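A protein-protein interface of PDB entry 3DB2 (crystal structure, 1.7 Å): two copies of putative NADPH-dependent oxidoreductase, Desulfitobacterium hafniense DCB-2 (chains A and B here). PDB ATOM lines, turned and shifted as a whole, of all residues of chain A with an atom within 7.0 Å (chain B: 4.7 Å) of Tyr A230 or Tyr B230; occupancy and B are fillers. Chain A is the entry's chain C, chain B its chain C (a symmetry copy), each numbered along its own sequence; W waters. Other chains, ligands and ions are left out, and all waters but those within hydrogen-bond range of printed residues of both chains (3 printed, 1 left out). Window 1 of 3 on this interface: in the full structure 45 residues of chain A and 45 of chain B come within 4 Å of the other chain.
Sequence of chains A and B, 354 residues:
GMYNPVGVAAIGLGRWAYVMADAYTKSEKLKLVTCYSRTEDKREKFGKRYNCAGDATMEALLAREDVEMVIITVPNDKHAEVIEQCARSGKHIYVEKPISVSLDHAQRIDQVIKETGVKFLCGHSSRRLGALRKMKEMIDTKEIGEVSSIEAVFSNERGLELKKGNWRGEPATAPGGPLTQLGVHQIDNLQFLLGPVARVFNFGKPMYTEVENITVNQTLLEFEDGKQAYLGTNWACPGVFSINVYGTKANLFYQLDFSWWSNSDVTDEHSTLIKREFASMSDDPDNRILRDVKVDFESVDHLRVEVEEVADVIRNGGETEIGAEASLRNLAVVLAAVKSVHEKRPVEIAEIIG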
ATOM      1  N   SER A 149      30.501   0.617   4.832  1.00  0.00           N
ATOM      2  CA  SER A 149      30.288   1.931   5.447  1.00  0.00           C
ATOM      3  C   SER A 149      30.495   1.874   6.968  1.00  0.00           C
ATOM      4  O   SER A 149      30.471   0.829   7.602  1.00  0.00           O
ATOM      5  CB  SER A 149      28.896   2.449   5.132  1.00  0.00           C
ATOM      6  OG  SER A 149      27.866   1.681   5.701  1.00  0.00           O
ATOM      7  N   ILE A 150      30.674   3.076   7.540  1.00  0.00           N
ATOM      8  CA  ILE A 150      30.804   3.259   8.973  1.00  0.00           C
ATOM      9  C   ILE A 150      29.932   4.447   9.387  1.00  0.00           C
ATOM     10  O   ILE A 150      29.807   5.395   8.638  1.00  0.00           O
ATOM     11  CB  ILE A 150      32.253   3.481   9.419  1.00  0.00           C
ATOM     12  CG1 ILE A 150      33.129   2.246   9.241  1.00  0.00           C
ATOM     13  CG2 ILE A 150      32.314   4.002  10.861  1.00  0.00           C
ATOM     14  CD1 ILE A 150      34.592   2.556   9.498  1.00  0.00           C
ATOM     15  N   GLU A 151      29.330   4.358  10.584  1.00  0.00           N
ATOM     16  CA  GLU A 151      28.598   5.485  11.142  1.00  0.00           C
ATOM     17  C   GLU A 151      29.198   5.823  12.514  1.00  0.00           C
ATOM     18  O   GLU A 151      29.247   4.914  13.328  1.00  0.00           O
ATOM     19  CB  GLU A 151      27.108   5.185  11.329  1.00  0.00           C
ATOM     20  CG  GLU A 151      26.472   4.724  10.034  1.00  0.00           C
ATOM     21  CD  GLU A 151      25.251   3.850  10.292  1.00  0.00           C
ATOM     22  OE1 GLU A 151      25.034   3.381  11.431  1.00  0.00           O
ATOM     23  OE2 GLU A 151      24.536   3.609   9.290  1.00  0.00           O
ATOM     24  N   ALA A 152      29.645   7.041  12.685  1.00  0.00           N
ATOM     25  CA  ALA A 152      30.315   7.478  13.905  1.00  0.00           C
ATOM     26  C   ALA A 152      29.513   8.630  14.501  1.00  0.00           C
ATOM     27  O   ALA A 152      28.971   9.434  13.730  1.00  0.00           O
ATOM     28  CB  ALA A 152      31.737   7.918  13.621  1.00  0.00           C
ATOM     29  N   VAL A 153      29.411   8.697  15.821  1.00  0.00           N
ATOM     30  CA  VAL A 153      28.649   9.783  16.433  1.00  0.00           C
ATOM     31  C   VAL A 153      29.430  10.281  17.648  1.00  0.00           C
ATOM     32  O   VAL A 153      29.957   9.451  18.380  1.00  0.00           O
ATOM     33  CB  VAL A 153      27.257   9.342  16.899  1.00  0.00           C
ATOM     34  CG1 VAL A 153      26.524  10.436  17.668  1.00  0.00           C
ATOM     35  CG2 VAL A 153      26.426   8.894  15.700  1.00  0.00           C
ATOM     36  N   LEU A 190      38.137   7.373  12.034  1.00  0.00           N
ATOM     37  CA  LEU A 190      37.688   6.951  10.708  1.00  0.00           C
ATOM     38  C   LEU A 190      38.835   6.744   9.734  1.00  0.00           C
ATOM     39  O   LEU A 190      38.876   5.800   8.952  1.00  0.00           O
ATOM     40  CB  LEU A 190      36.714   7.993  10.134  1.00  0.00           C
ATOM     41  CG  LEU A 190      35.315   7.956  10.776  1.00  0.00           C
ATOM     42  CD1 LEU A 190      34.511   9.203  10.428  1.00  0.00           C
ATOM     43  CD2 LEU A 190      34.586   6.703  10.328  1.00  0.00           C
ATOM     44  N   ASN A 217      25.736  18.905  13.285  1.00  0.00           N
ATOM     45  CA  ASN A 217      26.221  18.552  11.987  1.00  0.00           C
ATOM     46  C   ASN A 217      25.862  17.066  11.686  1.00  0.00           C
ATOM     47  O   ASN A 217      25.857  16.262  12.602  1.00  0.00           O
ATOM     48  CB  ASN A 217      27.720  18.642  11.760  1.00  0.00           C
ATOM     49  CG  ASN A 217      28.304  20.023  12.025  1.00  0.00           C
ATOM     50  OD1 ASN A 217      28.234  20.889  11.176  1.00  0.00           O
ATOM     51  ND2 ASN A 217      28.879  20.105  13.221  1.00  0.00           N
ATOM     52  N   GLN A 218      25.613  16.823  10.417  1.00  0.00           N
ATOM     53  CA  GLN A 218      25.644  15.469   9.865  1.00  0.00           C
ATOM     54  C   GLN A 218      26.550  15.556   8.628  1.00  0.00           C
ATOM     55  O   GLN A 218      26.287  16.323   7.718  1.00  0.00           O
ATOM     56  CB  GLN A 218      24.262  14.980   9.550  1.00  0.00           C
ATOM     57  CG  GLN A 218      23.500  14.658  10.832  1.00  0.00           C
ATOM     58  CD  GLN A 218      22.162  13.996  10.623  1.00  0.00           C
ATOM     59  OE1 GLN A 218      21.384  14.465   9.786  1.00  0.00           O
ATOM     60  NE2 GLN A 218      21.848  12.919  11.333  1.00  0.00           N
ATOM     61  N   THR A 219      27.586  14.725   8.624  1.00  0.00           N
ATOM     62  CA  THR A 219      28.628  14.810   7.615  1.00  0.00           C
ATOM     63  C   THR A 219      28.754  13.453   6.906  1.00  0.00           C
ATOM     64  O   THR A 219      28.820  12.461   7.657  1.00  0.00           O
ATOM     65  CB  THR A 219      29.993  15.147   8.240  1.00  0.00           C
ATOM     66  OG1 THR A 219      29.810  16.311   9.044  1.00  0.00           O
ATOM     67  CG2 THR A 219      30.995  15.433   7.141  1.00  0.00           C
ATOM     68  N   LEU A 220      28.793  13.513   5.591  1.00  0.00           N
ATOM     69  CA  LEU A 220      29.123  12.337   4.789  1.00  0.00           C
ATOM     70  C   LEU A 220      30.562  12.464   4.262  1.00  0.00           C
ATOM     71  O   LEU A 220      31.035  13.515   3.860  1.00  0.00           O
ATOM     72  CB  LEU A 220      28.175  12.165   3.617  1.00  0.00           C
ATOM     73  CG  LEU A 220      26.705  12.010   3.985  1.00  0.00           C
ATOM     74  CD1 LEU A 220      25.906  11.716   2.709  1.00  0.00           C
ATOM     75  CD2 LEU A 220      26.481  10.945   5.039  1.00  0.00           C
ATOM     76  N   LEU A 221      31.243  11.342   4.248  1.00  0.00           N
ATOM     77  CA  LEU A 221      32.589  11.157   3.756  1.00  0.00           C
ATOM     78  C   LEU A 221      32.642  10.034   2.726  1.00  0.00           C
ATOM     79  O   LEU A 221      31.985   9.011   2.857  1.00  0.00           O
ATOM     80  CB  LEU A 221      33.539  10.830   4.916  1.00  0.00           C
ATOM     81  CG  LEU A 221      33.326  11.662   6.188  1.00  0.00           C
ATOM     82  CD1 LEU A 221      33.428  10.787   7.425  1.00  0.00           C
ATOM     83  CD2 LEU A 221      34.333  12.791   6.248  1.00  0.00           C
ATOM     84  N   PHE A 223      35.815   7.798   1.003  1.00  0.00           N
ATOM     85  CA  PHE A 223      37.225   7.476   1.175  1.00  0.00           C
ATOM     86  C   PHE A 223      37.922   7.364  -0.185  1.00  0.00           C
ATOM     87  O   PHE A 223      37.246   7.239  -1.201  1.00  0.00           O
ATOM     88  CB  PHE A 223      37.418   6.178   1.993  1.00  0.00           C
ATOM     89  CG  PHE A 223      37.095   6.531   3.459  1.00  0.00           C
ATOM     90  CD1 PHE A 223      35.792   6.446   3.910  1.00  0.00           C
ATOM     91  CD2 PHE A 223      38.097   6.948   4.297  1.00  0.00           C
ATOM     92  CE1 PHE A 223      35.463   6.798   5.213  1.00  0.00           C
ATOM     93  CE2 PHE A 223      37.775   7.339   5.602  1.00  0.00           C
ATOM     94  CZ  PHE A 223      36.466   7.285   6.036  1.00  0.00           C
ATOM     95  N   GLN A 228      32.617   4.366   2.530  1.00  0.00           N
ATOM     96  CA  GLN A 228      31.877   5.561   2.909  1.00  0.00           C
ATOM     97  C   GLN A 228      31.692   5.675   4.416  1.00  0.00           C
ATOM     98  O   GLN A 228      31.736   4.650   5.096  1.00  0.00           O
ATOM     99  CB  GLN A 228      30.487   5.539   2.296  1.00  0.00           C
ATOM    100  CG  GLN A 228      30.493   5.632   0.792  1.00  0.00           C
ATOM    101  CD  GLN A 228      29.138   5.641   0.134  1.00  0.00           C
ATOM    102  OE1 GLN A 228      28.958   5.016  -0.922  1.00  0.00           O
ATOM    103  NE2 GLN A 228      28.184   6.370   0.709  1.00  0.00           N
ATOM    104  N   ALA A 229      31.487   6.890   4.903  1.00  0.00           N
ATOM    105  CA  ALA A 229      31.168   7.051   6.324  1.00  0.00           C
ATOM    106  C   ALA A 229      30.225   8.247   6.536  1.00  0.00           C
ATOM    107  O   ALA A 229      30.178   9.166   5.728  1.00  0.00           O
ATOM    108  CB  ALA A 229      32.403   7.197   7.174  1.00  0.00           C
ATOM    109  N   TYR A 230      29.500   8.151   7.642  1.00  0.00           N
ATOM    110  CA  TYR A 230      28.654   9.154   8.250  1.00  0.00           C
ATOM    111  C   TYR A 230      29.270   9.595   9.578  1.00  0.00           C
ATOM    112  O   TYR A 230      29.689   8.712  10.334  1.00  0.00           O
ATOM    113  CB  TYR A 230      27.252   8.582   8.490  1.00  0.00           C
ATOM    114  CG  TYR A 230      26.473   9.374   9.509  1.00  0.00           C
ATOM    115  CD1 TYR A 230      25.996  10.649   9.199  1.00  0.00           C
ATOM    116  CD2 TYR A 230      26.227   8.856  10.774  1.00  0.00           C
ATOM    117  CE1 TYR A 230      25.287  11.358  10.151  1.00  0.00           C
ATOM    118  CE2 TYR A 230      25.519   9.574  11.730  1.00  0.00           C
ATOM    119  CZ  TYR A 230      25.059  10.825  11.389  1.00  0.00           C
ATOM    120  OH  TYR A 230      24.347  11.589  12.294  1.00  0.00           O
ATOM    121  N   LEU A 231      29.301  10.907   9.820  1.00  0.00           N
ATOM    122  CA  LEU A 231      29.690  11.418  11.126  1.00  0.00           C
ATOM    123  C   LEU A 231      28.637  12.398  11.632  1.00  0.00           C
ATOM    124  O   LEU A 231      28.407  13.404  10.975  1.00  0.00           O
ATOM    125  CB  LEU A 231      31.050  12.092  11.047  1.00  0.00           C
ATOM    126  CG  LEU A 231      31.486  12.872  12.296  1.00  0.00           C
ATOM    127  CD1 LEU A 231      31.584  11.965  13.508  1.00  0.00           C
ATOM    128  CD2 LEU A 231      32.826  13.529  12.042  1.00  0.00           C
ATOM    129  N   GLY A 232      28.028  12.117  12.767  1.00  0.00           N
ATOM    130  CA  GLY A 232      27.102  13.035  13.422  1.00  0.00           C
ATOM    131  C   GLY A 232      27.796  13.657  14.616  1.00  0.00           C
ATOM    132  O   GLY A 232      28.415  12.948  15.404  1.00  0.00           O
ATOM    133  N   THR A 233      27.738  14.981  14.702  1.00  0.00           N
ATOM    134  CA  THR A 233      28.325  15.732  15.825  1.00  0.00           C
ATOM    135  C   THR A 233      27.235  16.673  16.328  1.00  0.00           C
ATOM    136  O   THR A 233      26.607  17.376  15.534  1.00  0.00           O
ATOM    137  CB  THR A 233      29.591  16.510  15.458  1.00  0.00           C
ATOM    138  OG1 THR A 233      29.400  17.245  14.246  1.00  0.00           O
ATOM    139  CG2 THR A 233      30.752  15.548  15.245  1.00  0.00           C
ATOM    140  N   TYR A 246      29.887  -1.723   9.188  1.00  0.00           N
ATOM    141  CA  TYR A 246      29.110  -2.680   8.416  1.00  0.00           C
ATOM    142  C   TYR A 246      30.067  -3.445   7.495  1.00  0.00           C
ATOM    143  O   TYR A 246      30.717  -2.793   6.666  1.00  0.00           O
ATOM    144  CB  TYR A 246      28.051  -1.931   7.602  1.00  0.00           C
ATOM    145  CG  TYR A 246      27.117  -1.188   8.550  1.00  0.00           C
ATOM    146  CD1 TYR A 246      26.114  -1.870   9.222  1.00  0.00           C
ATOM    147  CD2 TYR A 246      27.237   0.178   8.792  1.00  0.00           C
ATOM    148  CE1 TYR A 246      25.263  -1.208  10.087  1.00  0.00           C
ATOM    149  CE2 TYR A 246      26.366   0.818   9.660  1.00  0.00           C
ATOM    150  CZ  TYR A 246      25.375   0.142  10.319  1.00  0.00           C
ATOM    151  OH  TYR A 246      24.488   0.767  11.210  1.00  0.00           O
ATOM    152  N   ILE B 150      18.049  12.730  13.486  1.00  0.00           N
ATOM    153  CA  ILE B 150      17.683  11.327  13.530  1.00  0.00           C
ATOM    154  C   ILE B 150      18.635  10.552  12.616  1.00  0.00           C
ATOM    155  O   ILE B 150      19.044  11.066  11.594  1.00  0.00           O
ATOM    156  CB  ILE B 150      16.228  11.075  13.119  1.00  0.00           C
ATOM    157  CG1 ILE B 150      15.220  11.633  14.119  1.00  0.00           C
ATOM    158  CG2 ILE B 150      15.979   9.585  12.851  1.00  0.00           C
ATOM    159  CD1 ILE B 150      13.801  11.548  13.588  1.00  0.00           C
ATOM    160  N   GLU B 151      18.980   9.319  13.020  1.00  0.00           N
ATOM    161  CA  GLU B 151      19.760   8.439  12.164  1.00  0.00           C
ATOM    162  C   GLU B 151      18.973   7.137  11.958  1.00  0.00           C
ATOM    163  O   GLU B 151      18.631   6.540  12.968  1.00  0.00           O
ATOM    164  CB  GLU B 151      21.123   8.087  12.766  1.00  0.00           C
ATOM    165  CG  GLU B 151      21.912   9.334  13.109  1.00  0.00           C
ATOM    166  CD  GLU B 151      22.912   9.071  14.228  1.00  0.00           C
ATOM    167  OE1 GLU B 151      22.836   8.030  14.917  1.00  0.00           O
ATOM    168  OE2 GLU B 151      23.756   9.978  14.424  1.00  0.00           O
ATOM    169  N   ALA B 152      18.696   6.795  10.726  1.00  0.00           N
ATOM    170  CA  ALA B 152      17.885   5.631  10.386  1.00  0.00           C
ATOM    171  C   ALA B 152      18.729   4.699   9.525  1.00  0.00           C
ATOM    172  O   ALA B 152      19.525   5.198   8.717  1.00  0.00           O
ATOM    173  CB  ALA B 152      16.627   6.039   9.645  1.00  0.00           C
ATOM    174  N   VAL B 153      18.591   3.393   9.705  1.00  0.00           N
ATOM    175  CA  VAL B 153      19.383   2.464   8.903  1.00  0.00           C
ATOM    176  C   VAL B 153      18.474   1.310   8.483  1.00  0.00           C
ATOM    177  O   VAL B 153      17.697   0.851   9.312  1.00  0.00           O
ATOM    178  CB  VAL B 153      20.577   1.886   9.671  1.00  0.00           C
ATOM    179  CG1 VAL B 153      21.313   0.808   8.882  1.00  0.00           C
ATOM    180  CG2 VAL B 153      21.540   3.007  10.055  1.00  0.00           C
ATOM    181  N   GLN B 218      24.550   6.394   1.635  1.00  0.00           N
ATOM    182  CA  GLN B 218      24.414   7.205   2.843  1.00  0.00           C
ATOM    183  C   GLN B 218      23.781   8.524   2.378  1.00  0.00           C
ATOM    184  O   GLN B 218      24.326   9.209   1.530  1.00  0.00           O
ATOM    185  CB  GLN B 218      25.738   7.394   3.523  1.00  0.00           C
ATOM    186  CG  GLN B 218      26.186   6.100   4.197  1.00  0.00           C
ATOM    187  CD  GLN B 218      27.420   6.228   5.052  1.00  0.00           C
ATOM    188  OE1 GLN B 218      28.405   6.823   4.602  1.00  0.00           O
ATOM    189  NE2 GLN B 218      27.424   5.710   6.274  1.00  0.00           N
ATOM    190  N   THR B 219      22.649   8.856   2.985  1.00  0.00           N
ATOM    191  CA  THR B 219      21.840   9.977   2.535  1.00  0.00           C
ATOM    192  C   THR B 219      21.641  10.956   3.703  1.00  0.00           C
ATOM    193  O   THR B 219      21.282  10.439   4.778  1.00  0.00           O
ATOM    194  CB  THR B 219      20.452   9.516   2.059  1.00  0.00           C
ATOM    195  OG1 THR B 219      20.659   8.475   1.106  1.00  0.00           O
ATOM    196  CG2 THR B 219      19.731  10.677   1.406  1.00  0.00           C
ATOM    197  N   LEU B 220      21.860  12.221   3.412  1.00  0.00           N
ATOM    198  CA  LEU B 220      21.507  13.284   4.350  1.00  0.00           C
ATOM    199  C   LEU B 220      20.231  13.992   3.867  1.00  0.00           C
ATOM    200  O   LEU B 220      20.011  14.242   2.692  1.00  0.00           O
ATOM    201  CB  LEU B 220      22.620  14.306   4.494  1.00  0.00           C
ATOM    202  CG  LEU B 220      23.953  13.753   4.982  1.00  0.00           C
ATOM    203  CD1 LEU B 220      24.922  14.923   5.198  1.00  0.00           C
ATOM    204  CD2 LEU B 220      23.807  12.913   6.235  1.00  0.00           C
ATOM    205  N   GLN B 228      17.307  17.617  11.015  1.00  0.00           N
ATOM    206  CA  GLN B 228      18.138  16.895  10.064  1.00  0.00           C
ATOM    207  C   GLN B 228      18.052  15.385  10.246  1.00  0.00           C
ATOM    208  O   GLN B 228      17.723  14.941  11.346  1.00  0.00           O
ATOM    209  CB  GLN B 228      19.598  17.277  10.241  1.00  0.00           C
ATOM    210  CG  GLN B 228      19.889  18.713   9.893  1.00  0.00           C
ATOM    211  CD  GLN B 228      21.329  19.137  10.026  1.00  0.00           C
ATOM    212  OE1 GLN B 228      21.605  20.257  10.483  1.00  0.00           O
ATOM    213  NE2 GLN B 228      22.259  18.286   9.599  1.00  0.00           N
ATOM    214  N   ALA B 229      18.348  14.638   9.193  1.00  0.00           N
ATOM    215  CA  ALA B 229      18.416  13.181   9.341  1.00  0.00           C
ATOM    216  C   ALA B 229      19.476  12.590   8.397  1.00  0.00           C
ATOM    217  O   ALA B 229      19.816  13.178   7.379  1.00  0.00           O
ATOM    218  CB  ALA B 229      17.081  12.522   9.113  1.00  0.00           C
ATOM    219  N   TYR B 230      19.957  11.426   8.816  1.00  0.00           N
ATOM    220  CA  TYR B 230      20.818  10.505   8.110  1.00  0.00           C
ATOM    221  C   TYR B 230      20.040   9.228   7.794  1.00  0.00           C
ATOM    222  O   TYR B 230      19.354   8.740   8.698  1.00  0.00           O
ATOM    223  CB  TYR B 230      22.045  10.171   8.966  1.00  0.00           C
ATOM    224  CG  TYR B 230      22.731   8.906   8.521  1.00  0.00           C
ATOM    225  CD1 TYR B 230      23.450   8.875   7.325  1.00  0.00           C
ATOM    226  CD2 TYR B 230      22.651   7.748   9.286  1.00  0.00           C
ATOM    227  CE1 TYR B 230      24.068   7.701   6.936  1.00  0.00           C
ATOM    228  CE2 TYR B 230      23.270   6.569   8.888  1.00  0.00           C
ATOM    229  CZ  TYR B 230      23.975   6.575   7.706  1.00  0.00           C
ATOM    230  OH  TYR B 230      24.613   5.436   7.255  1.00  0.00           O
ATOM    231  N   LEU B 231      20.168   8.734   6.561  1.00  0.00           N
ATOM    232  CA  LEU B 231      19.624   7.429   6.217  1.00  0.00           C
ATOM    233  C   LEU B 231      20.703   6.578   5.554  1.00  0.00           C
ATOM    234  O   LEU B 231      21.205   6.976   4.511  1.00  0.00           O
ATOM    235  CB  LEU B 231      18.425   7.581   5.296  1.00  0.00           C
ATOM    236  CG  LEU B 231      17.889   6.283   4.673  1.00  0.00           C
ATOM    237  CD1 LEU B 231      17.425   5.309   5.740  1.00  0.00           C
ATOM    238  CD2 LEU B 231      16.738   6.605   3.743  1.00  0.00           C
ATOM    239  N   GLY B 232      21.037   5.443   6.134  1.00  0.00           N
ATOM    240  CA  GLY B 232      21.954   4.481   5.533  1.00  0.00           C
ATOM    241  C   GLY B 232      21.153   3.309   5.006  1.00  0.00           C
ATOM    242  O   GLY B 232      20.294   2.786   5.710  1.00  0.00           O
HETATM  243  O   HOH W   1      24.405   2.142   7.057  1.00  0.00           O
HETATM  244  O   HOH W   2      21.350  16.091   7.647  1.00  0.00           O
HETATM  245  O   HOH W   3      24.075  12.413  15.485  1.00  0.00           O
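Among the printed residues, pairs that only touch across the chains: Glu A151 with Val B153, Val A153 with Glu B151, Leu A220 with Gln B218, Gln A218 with Leu B220, Gln A228 with Gln B218, Gln A218 with Gln B228, Leu A220 with Leu B220, Tyr A230 with Tyr B230, Ser A149 with Gln B218 and Tyr A246 with Val B153.
Water W3 lies within hydrogen-bond range of OE2 of Glu B151 and OH of Tyr A230.
Water W1 bridges the side-chain carboxylate (OE2) of Glu A151 (2.7 Å) and the side-chain hydroxyl (OH) of Tyr B230 (3.3 Å).
Water W2 lies within hydrogen-bond range of OE1 of Gln A218, NE2 of Gln B228 and O of Ala B229.
Ile A150 touches Gln B218, and with the chains exchanged Gln A218 touches Ile B150.
Glu A151 touches Val B153, and with the chains exchanged Val A153 touches Glu B151.
Gln A218 touches Ala B229, and with the chains exchanged Ala A229 touches Gln B218.
Leu B220 touches its own counterpart, Leu A220.
12 positions are printed for both chains.
Of the 18 pairs that touch across the chains among the printed residues, 16 have their exchanged pair printed and touching as well.
Printed residues of chain B within 4 Å of Ile A150: Gln B218 (3.4 Å).
Thr A219 touches none of the printed residues of chain B.
Of the printed residues of chain B, Leu A220 touches Gln B218 and Leu B220.
Of the printed residues of chain B, Tyr A230 touches Glu B151 (2.7 Å), Gln B218 (3.5 Å) and Tyr B230 (3.6 Å).
Of the printed residues of chain A, Ile B150 touches Gln A218 (3.4 Å).
Printed residues of chain A within 4 Å of Gln B218: Ser A149, Ile A150, Leu A220, Gln A228, Ala A229 and Tyr A230.
Thr B219 touches none of the printed residues of chain A.
Of the printed residues of chain A, Tyr B230 touches Glu A151 (2.7 Å), Gln A218 (3.5 Å) and Tyr A230 (3.6 Å).
The nearest residue of chain B that does not touch Tyr A230 is Leu B220 (4.3 Å).
The nearest printed residue of chain A that does not touch Ile B150 is Tyr A230 (5.4 Å).
Hydrophobic or aromatic side chains of chain B within 4 Å of the printed part of chain A: Val B153, Leu B220 and Tyr B230.
Along chain B the printed residues that touch a printed residue of chain A span positions 150 to 230.
Printed residues of chain A that touch a printed residue of chain B: Ser A149, Ile A150, Glu A151, Val A153, Gln A218, Leu A220, Gln A228, Ala A229, Tyr A230 and Tyr A246.
Hydrophobic or aromatic side chains of chain A that line the printed part of chain B: Val A153, Leu A220, Tyr A230 and Tyr A246.
Among the printed residues, no Asp or Glu carboxylate lies within 4 Å of a Lys or Arg side-chain nitrogen of the other chain.
The side-chain amide nitrogen (NE2) of Gln B218 lies within hydrogen-bond range of the backbone carbonyl oxygen (O) of Ile A150.
The side-chain carboxylate of Glu A151 lies within hydrogen-bond range of the side-chain hydroxyl of Tyr B230.
NE2 of Gln A218 lies within hydrogen-bond range of O of Ile B150 (3.4 Å).
The side-chain amide oxygen of Gln A218 lies close to the backbone NH of Ala B229 (3.1 Å).
The side-chain amide nitrogen (NE2) of Gln A218 sits close to the backbone NH (N) of Tyr B230, at 3.5 Å.
The side-chain amide oxygen (OE1) of Gln B218 lies close to the backbone NH (N) of Ala A229 (3.1 Å).
OE2 of Glu B151 is in hydrogen-bond range of OH of Tyr A230 (2.7 Å).
N of Tyr A230 sits close to NE2 of Gln B218 (3.5 Å).
The backbone carbonyl oxygen (O) of Ser A149 sits at hydrogen-bond distance from the backbone NH (N) of Tyr A246.
O of Gln A228 lies within hydrogen-bond range of N of Ile A150 (3.1 Å).
The backbone NH of Tyr A230 lies within hydrogen-bond range of the backbone carbonyl oxygen of Ile A150 (2.9 Å).
The side-chain amide nitrogen (NE2) of Gln A218 is in hydrogen-bond range of the side-chain hydroxyl (OH) of Tyr A230 (3.0 Å).
The backbone NH (N) of Leu A221 is in hydrogen-bond range of the backbone carbonyl oxygen (O) of Ala A229 (2.8 Å).
O of Ile B150 sits at hydrogen-bond distance from N of Tyr B230 (2.9 Å).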
